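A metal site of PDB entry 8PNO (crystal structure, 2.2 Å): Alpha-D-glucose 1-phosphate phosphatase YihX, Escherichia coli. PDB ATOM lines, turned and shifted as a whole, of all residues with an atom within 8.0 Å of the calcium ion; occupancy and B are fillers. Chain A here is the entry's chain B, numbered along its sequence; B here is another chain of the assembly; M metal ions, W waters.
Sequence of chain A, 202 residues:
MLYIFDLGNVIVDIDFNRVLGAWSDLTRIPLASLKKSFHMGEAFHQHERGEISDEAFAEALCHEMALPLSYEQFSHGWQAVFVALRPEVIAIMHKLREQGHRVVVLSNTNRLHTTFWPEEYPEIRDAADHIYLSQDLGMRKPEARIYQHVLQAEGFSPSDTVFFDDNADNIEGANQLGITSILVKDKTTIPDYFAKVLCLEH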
ATOM      1  N   GLN A  79       9.553 -29.018  -6.990  1.00  0.00           N
ATOM      2  CA  GLN A  79       8.378 -28.471  -7.652  1.00  0.00           C
ATOM      3  C   GLN A  79       7.924 -29.279  -8.889  1.00  0.00           C
ATOM      4  O   GLN A  79       6.766 -29.141  -9.324  1.00  0.00           O
ATOM      5  CB  GLN A  79       8.653 -27.026  -8.051  1.00  0.00           C
ATOM      6  CG  GLN A  79       7.447 -26.317  -8.641  1.00  0.00           C
ATOM      7  CD  GLN A  79       6.323 -26.187  -7.635  1.00  0.00           C
ATOM      8  OE1 GLN A  79       6.359 -25.303  -6.777  1.00  0.00           O
ATOM      9  NE2 GLN A  79       5.361 -27.091  -7.741  1.00  0.00           N
ATOM     10  N   ARG A 111       5.699 -30.863   1.479  1.00  0.00           N
ATOM     11  CA  ARG A 111       5.605 -29.527   0.935  1.00  0.00           C
ATOM     12  C   ARG A 111       6.767 -28.728   1.531  1.00  0.00           C
ATOM     13  O   ARG A 111       7.196 -28.983   2.656  1.00  0.00           O
ATOM     14  CB  ARG A 111       4.265 -28.880   1.307  1.00  0.00           C
ATOM     15  CG  ARG A 111       4.132 -27.422   0.874  1.00  0.00           C
ATOM     16  CD  ARG A 111       2.862 -26.665   1.248  1.00  0.00           C
ATOM     17  NE  ARG A 111       2.760 -26.306   2.666  1.00  0.00           N
ATOM     18  CZ  ARG A 111       2.317 -27.124   3.609  1.00  0.00           C
ATOM     19  NH1 ARG A 111       2.442 -26.803   4.881  1.00  0.00           N
ATOM     20  NH2 ARG A 111       1.817 -28.295   3.269  1.00  0.00           N
ATOM     21  N   LEU A 112       7.249 -27.765   0.760  1.00  0.00           N
ATOM     22  CA  LEU A 112       8.172 -26.776   1.259  1.00  0.00           C
ATOM     23  C   LEU A 112       7.464 -25.424   1.242  1.00  0.00           C
ATOM     24  O   LEU A 112       6.502 -25.240   0.499  1.00  0.00           O
ATOM     25  CB  LEU A 112       9.405 -26.782   0.328  1.00  0.00           C
ATOM     26  CG  LEU A 112      10.021 -28.139  -0.058  1.00  0.00           C
ATOM     27  CD1 LEU A 112      11.181 -27.944  -1.027  1.00  0.00           C
ATOM     28  CD2 LEU A 112      10.519 -28.908   1.159  1.00  0.00           C
ATOM     29  N   HIS A 113       7.989 -24.459   1.998  1.00  0.00           N
ATOM     30  CA  HIS A 113       7.454 -23.103   1.980  1.00  0.00           C
ATOM     31  C   HIS A 113       7.578 -22.466   0.601  1.00  0.00           C
ATOM     32  O   HIS A 113       6.903 -21.464   0.365  1.00  0.00           O
ATOM     33  CB  HIS A 113       8.117 -22.163   2.983  1.00  0.00           C
ATOM     34  CG  HIS A 113       9.558 -21.760   2.743  1.00  0.00           C
ATOM     35  ND1 HIS A 113      10.651 -22.580   2.968  1.00  0.00           N
ATOM     36  CD2 HIS A 113      10.064 -20.550   2.396  1.00  0.00           C
ATOM     37  CE1 HIS A 113      11.763 -21.895   2.723  1.00  0.00           C
ATOM     38  NE2 HIS A 113      11.436 -20.653   2.389  1.00  0.00           N
ATOM     39  N   THR A 114       8.445 -22.966  -0.297  1.00  0.00           N
ATOM     40  CA  THR A 114       8.615 -22.359  -1.622  1.00  0.00           C
ATOM     41  C   THR A 114       7.897 -23.144  -2.726  1.00  0.00           C
ATOM     42  O   THR A 114       7.909 -22.683  -3.864  1.00  0.00           O
ATOM     43  CB  THR A 114      10.085 -22.237  -2.000  1.00  0.00           C
ATOM     44  OG1 THR A 114      10.655 -23.490  -1.628  1.00  0.00           O
ATOM     45  CG2 THR A 114      10.771 -21.060  -1.328  1.00  0.00           C
ATOM     46  N   THR A 115       7.289 -24.294  -2.412  1.00  0.00           N
ATOM     47  CA  THR A 115       6.608 -25.070  -3.430  1.00  0.00           C
ATOM     48  C   THR A 115       5.075 -24.984  -3.363  1.00  0.00           C
ATOM     49  O   THR A 115       4.451 -24.877  -2.307  1.00  0.00           O
ATOM     50  CB  THR A 115       7.001 -26.551  -3.387  1.00  0.00           C
ATOM     51  OG1 THR A 115       6.448 -27.091  -2.195  1.00  0.00           O
ATOM     52  CG2 THR A 115       8.505 -26.752  -3.501  1.00  0.00           C
ATOM     53  N   PHE A 116       4.485 -25.077  -4.557  1.00  0.00           N
ATOM     54  CA  PHE A 116       3.049 -25.172  -4.750  1.00  0.00           C
ATOM     55  C   PHE A 116       2.704 -26.657  -4.791  1.00  0.00           C
ATOM     56  O   PHE A 116       3.204 -27.370  -5.662  1.00  0.00           O
ATOM     57  CB  PHE A 116       2.640 -24.371  -6.000  1.00  0.00           C
ATOM     58  CG  PHE A 116       1.189 -24.523  -6.379  1.00  0.00           C
ATOM     59  CD1 PHE A 116       0.180 -24.227  -5.481  1.00  0.00           C
ATOM     60  CD2 PHE A 116       0.832 -24.989  -7.644  1.00  0.00           C
ATOM     61  CE1 PHE A 116      -1.146 -24.388  -5.829  1.00  0.00           C
ATOM     62  CE2 PHE A 116      -0.508 -25.133  -7.998  1.00  0.00           C
ATOM     63  CZ  PHE A 116      -1.490 -24.820  -7.096  1.00  0.00           C
ATOM     64  N   TRP A 117       1.873 -27.123  -3.837  1.00  0.00           N
ATOM     65  CA  TRP A 117       1.745 -28.539  -3.557  1.00  0.00           C
ATOM     66  C   TRP A 117       0.271 -28.898  -3.604  1.00  0.00           C
ATOM     67  O   TRP A 117      -0.557 -28.011  -3.394  1.00  0.00           O
ATOM     68  CB  TRP A 117       2.400 -28.831  -2.187  1.00  0.00           C
ATOM     69  CG  TRP A 117       3.274 -30.053  -2.074  1.00  0.00           C
ATOM     70  CD1 TRP A 117       3.107 -31.090  -1.200  1.00  0.00           C
ATOM     71  CD2 TRP A 117       4.496 -30.325  -2.764  1.00  0.00           C
ATOM     72  NE1 TRP A 117       4.098 -32.009  -1.349  1.00  0.00           N
ATOM     73  CE2 TRP A 117       4.977 -31.566  -2.293  1.00  0.00           C
ATOM     74  CE3 TRP A 117       5.238 -29.643  -3.747  1.00  0.00           C
ATOM     75  CZ2 TRP A 117       6.148 -32.151  -2.771  1.00  0.00           C
ATOM     76  CZ3 TRP A 117       6.402 -30.226  -4.218  1.00  0.00           C
ATOM     77  CH2 TRP A 117       6.816 -31.484  -3.758  1.00  0.00           C
ATOM     78  N   GLU A 119      -2.174 -30.215  -1.631  1.00  0.00           N
ATOM     79  CA  GLU A 119      -3.058 -29.725  -0.589  1.00  0.00           C
ATOM     80  C   GLU A 119      -3.383 -28.233  -0.758  1.00  0.00           C
ATOM     81  O   GLU A 119      -4.274 -27.716  -0.085  1.00  0.00           O
ATOM     82  CB  GLU A 119      -2.450 -29.895   0.815  1.00  0.00           C
ATOM     83  CG  GLU A 119      -1.052 -29.302   0.977  1.00  0.00           C
ATOM     84  CD  GLU A 119       0.048 -30.328   0.788  1.00  0.00           C
ATOM     85  OE1 GLU A 119      -0.087 -31.207  -0.119  1.00  0.00           O
ATOM     86  OE2 GLU A 119       1.027 -30.257   1.566  1.00  0.00           O
ATOM     87  N   GLU A 120      -2.626 -27.538  -1.621  1.00  0.00           N
ATOM     88  CA  GLU A 120      -2.915 -26.132  -1.876  1.00  0.00           C
ATOM     89  C   GLU A 120      -3.744 -25.956  -3.143  1.00  0.00           C
ATOM     90  O   GLU A 120      -4.150 -24.855  -3.460  1.00  0.00           O
ATOM     91  CB  GLU A 120      -1.632 -25.315  -2.009  1.00  0.00           C
ATOM     92  CG  GLU A 120      -0.668 -25.505  -0.869  1.00  0.00           C
ATOM     93  CD  GLU A 120       0.592 -24.665  -1.060  1.00  0.00           C
ATOM     94  OE1 GLU A 120       1.257 -24.832  -2.111  1.00  0.00           O
ATOM     95  OE2 GLU A 120       0.865 -23.813  -0.201  1.00  0.00           O
ATOM     96  N   ARG A 125      -8.905 -28.245  -2.075  1.00  0.00           N
ATOM     97  CA  ARG A 125      -9.460 -27.531  -0.944  1.00  0.00           C
ATOM     98  C   ARG A 125     -10.989 -27.524  -0.968  1.00  0.00           C
ATOM     99  O   ARG A 125     -11.615 -27.700   0.077  1.00  0.00           O
ATOM    100  CB  ARG A 125      -8.926 -26.100  -0.881  1.00  0.00           C
ATOM    101  CG  ARG A 125      -7.456 -25.976  -0.514  1.00  0.00           C
ATOM    102  CD  ARG A 125      -7.142 -24.501  -0.272  1.00  0.00           C
ATOM    103  NE  ARG A 125      -5.925 -24.288   0.492  1.00  0.00           N
ATOM    104  CZ  ARG A 125      -4.919 -23.468   0.138  1.00  0.00           C
ATOM    105  NH1 ARG A 125      -5.036 -22.681  -0.929  1.00  0.00           N
ATOM    106  NH2 ARG A 125      -3.812 -23.423   0.858  1.00  0.00           N
ATOM    107  N   GLY B  21      -1.124 -21.341 -11.245  1.00  0.00           N
ATOM    108  CA  GLY B  21      -1.337 -21.814  -9.888  1.00  0.00           C
ATOM    109  C   GLY B  21      -0.149 -21.595  -8.956  1.00  0.00           C
ATOM    110  O   GLY B  21      -0.276 -20.974  -7.909  1.00  0.00           O
ATOM    111  N   ALA B  22       1.001 -22.117  -9.367  1.00  0.00           N
ATOM    112  CA  ALA B  22       2.226 -21.977  -8.594  1.00  0.00           C
ATOM    113  C   ALA B  22       2.588 -20.500  -8.393  1.00  0.00           C
ATOM    114  O   ALA B  22       3.126 -20.123  -7.351  1.00  0.00           O
ATOM    115  CB  ALA B  22       3.349 -22.743  -9.279  1.00  0.00           C
ATOM    116  N   SER B  24       0.360 -17.974  -8.407  1.00  0.00           N
ATOM    117  CA  SER B  24      -0.620 -17.438  -7.499  1.00  0.00           C
ATOM    118  C   SER B  24      -0.259 -17.841  -6.065  1.00  0.00           C
ATOM    119  O   SER B  24      -0.486 -17.079  -5.123  1.00  0.00           O
ATOM    120  CB  SER B  24      -2.022 -17.865  -7.860  1.00  0.00           C
ATOM    121  OG  SER B  24      -2.968 -17.403  -6.877  1.00  0.00           O
ATOM    122  N   ASP B  25       0.307 -19.048  -5.897  1.00  0.00           N
ATOM    123  CA  ASP B  25       0.680 -19.548  -4.594  1.00  0.00           C
ATOM    124  C   ASP B  25       1.821 -18.698  -4.025  1.00  0.00           C
ATOM    125  O   ASP B  25       1.739 -18.283  -2.879  1.00  0.00           O
ATOM    126  CB  ASP B  25       1.021 -21.042  -4.664  1.00  0.00           C
ATOM    127  CG  ASP B  25       1.669 -21.631  -3.415  1.00  0.00           C
ATOM    128  OD1 ASP B  25       0.953 -21.910  -2.463  1.00  0.00           O
ATOM    129  OD2 ASP B  25       2.888 -21.848  -3.427  1.00  0.00           O
ATOM    130  N   LEU B  26       2.875 -18.416  -4.801  1.00  0.00           N
ATOM    131  CA  LEU B  26       3.939 -17.547  -4.293  1.00  0.00           C
ATOM    132  C   LEU B  26       3.454 -16.104  -4.163  1.00  0.00           C
ATOM    133  O   LEU B  26       3.614 -15.505  -3.117  1.00  0.00           O
ATOM    134  CB  LEU B  26       5.177 -17.622  -5.192  1.00  0.00           C
ATOM    135  CG  LEU B  26       6.359 -16.740  -4.739  1.00  0.00           C
ATOM    136  CD1 LEU B  26       6.881 -17.116  -3.354  1.00  0.00           C
ATOM    137  CD2 LEU B  26       7.491 -16.779  -5.761  1.00  0.00           C
ATOM    138  N   ARG B  28       0.405 -14.566  -4.347  1.00  0.00           N
ATOM    139  CA  ARG B  28      -0.877 -14.288  -3.728  1.00  0.00           C
ATOM    140  C   ARG B  28      -1.754 -13.482  -4.696  1.00  0.00           C
ATOM    141  O   ARG B  28      -2.784 -12.939  -4.299  1.00  0.00           O
ATOM    142  CB  ARG B  28      -0.713 -13.519  -2.396  1.00  0.00           C
ATOM    143  CG  ARG B  28       0.316 -14.091  -1.418  1.00  0.00           C
ATOM    144  CD  ARG B  28      -0.276 -15.148  -0.509  1.00  0.00           C
ATOM    145  NE  ARG B  28      -0.427 -16.439  -1.174  1.00  0.00           N
ATOM    146  CZ  ARG B  28      -1.250 -17.419  -0.785  1.00  0.00           C
ATOM    147  NH1 ARG B  28      -2.132 -17.182   0.181  1.00  0.00           N
ATOM    148  NH2 ARG B  28      -1.204 -18.599  -1.378  1.00  0.00           N
HETATM  149 CA    CA M   1       2.906 -23.028  -1.272  1.00  0.00          CA
HETATM  150  O   HOH W   1       4.595 -21.382  -1.458  1.00  0.00           O
HETATM  151  O   HOH W   2       2.765 -20.762   0.258  1.00  0.00           O
HETATM  152  O   HOH W   3       4.388 -23.944   0.749  1.00  0.00           O
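The calcium ion is bound by water W1 (2.4 Å), OE2 of Glu 120 (2.4 Å), OD2 of Asp 25 of chain B (2.5 Å), OD1 of Asp 25 of chain B (2.5 Å), OE1 of Glu 120 (2.6 Å), O of Thr 115 (2.6 Å), water W3 (2.7 Å) and water W2 (2.7 Å).
The calcium ion has eight donor atoms within binding distance.
Three residues have an atom within 4 Å of the calcium ion: Thr 115, Glu 120 and Asp 25 of chain B.
The nearest printed residue that does not touch the calcium ion is Phe 116 (4.1 Å).
Water W3 lies within hydrogen-bond range of O of Leu 112 and NE of Arg 111.
The side-chain carboxylate (OE1) of Glu 120 sits close to the backbone NH (N) of Trp 117, 2.9 Å away.
NH1 of Arg 125 sits at hydrogen-bond distance from O of Glu 120, at 3.5 Å.
O of Asp 25 of chain B sits at hydrogen-bond distance from NE of Arg 28 of chain B, at 3.3 Å.
The backbone NH (N) of Leu 112 is in hydrogen-bond range of the side-chain hydroxyl (OG1) of Thr 115, 3.1 Å away.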
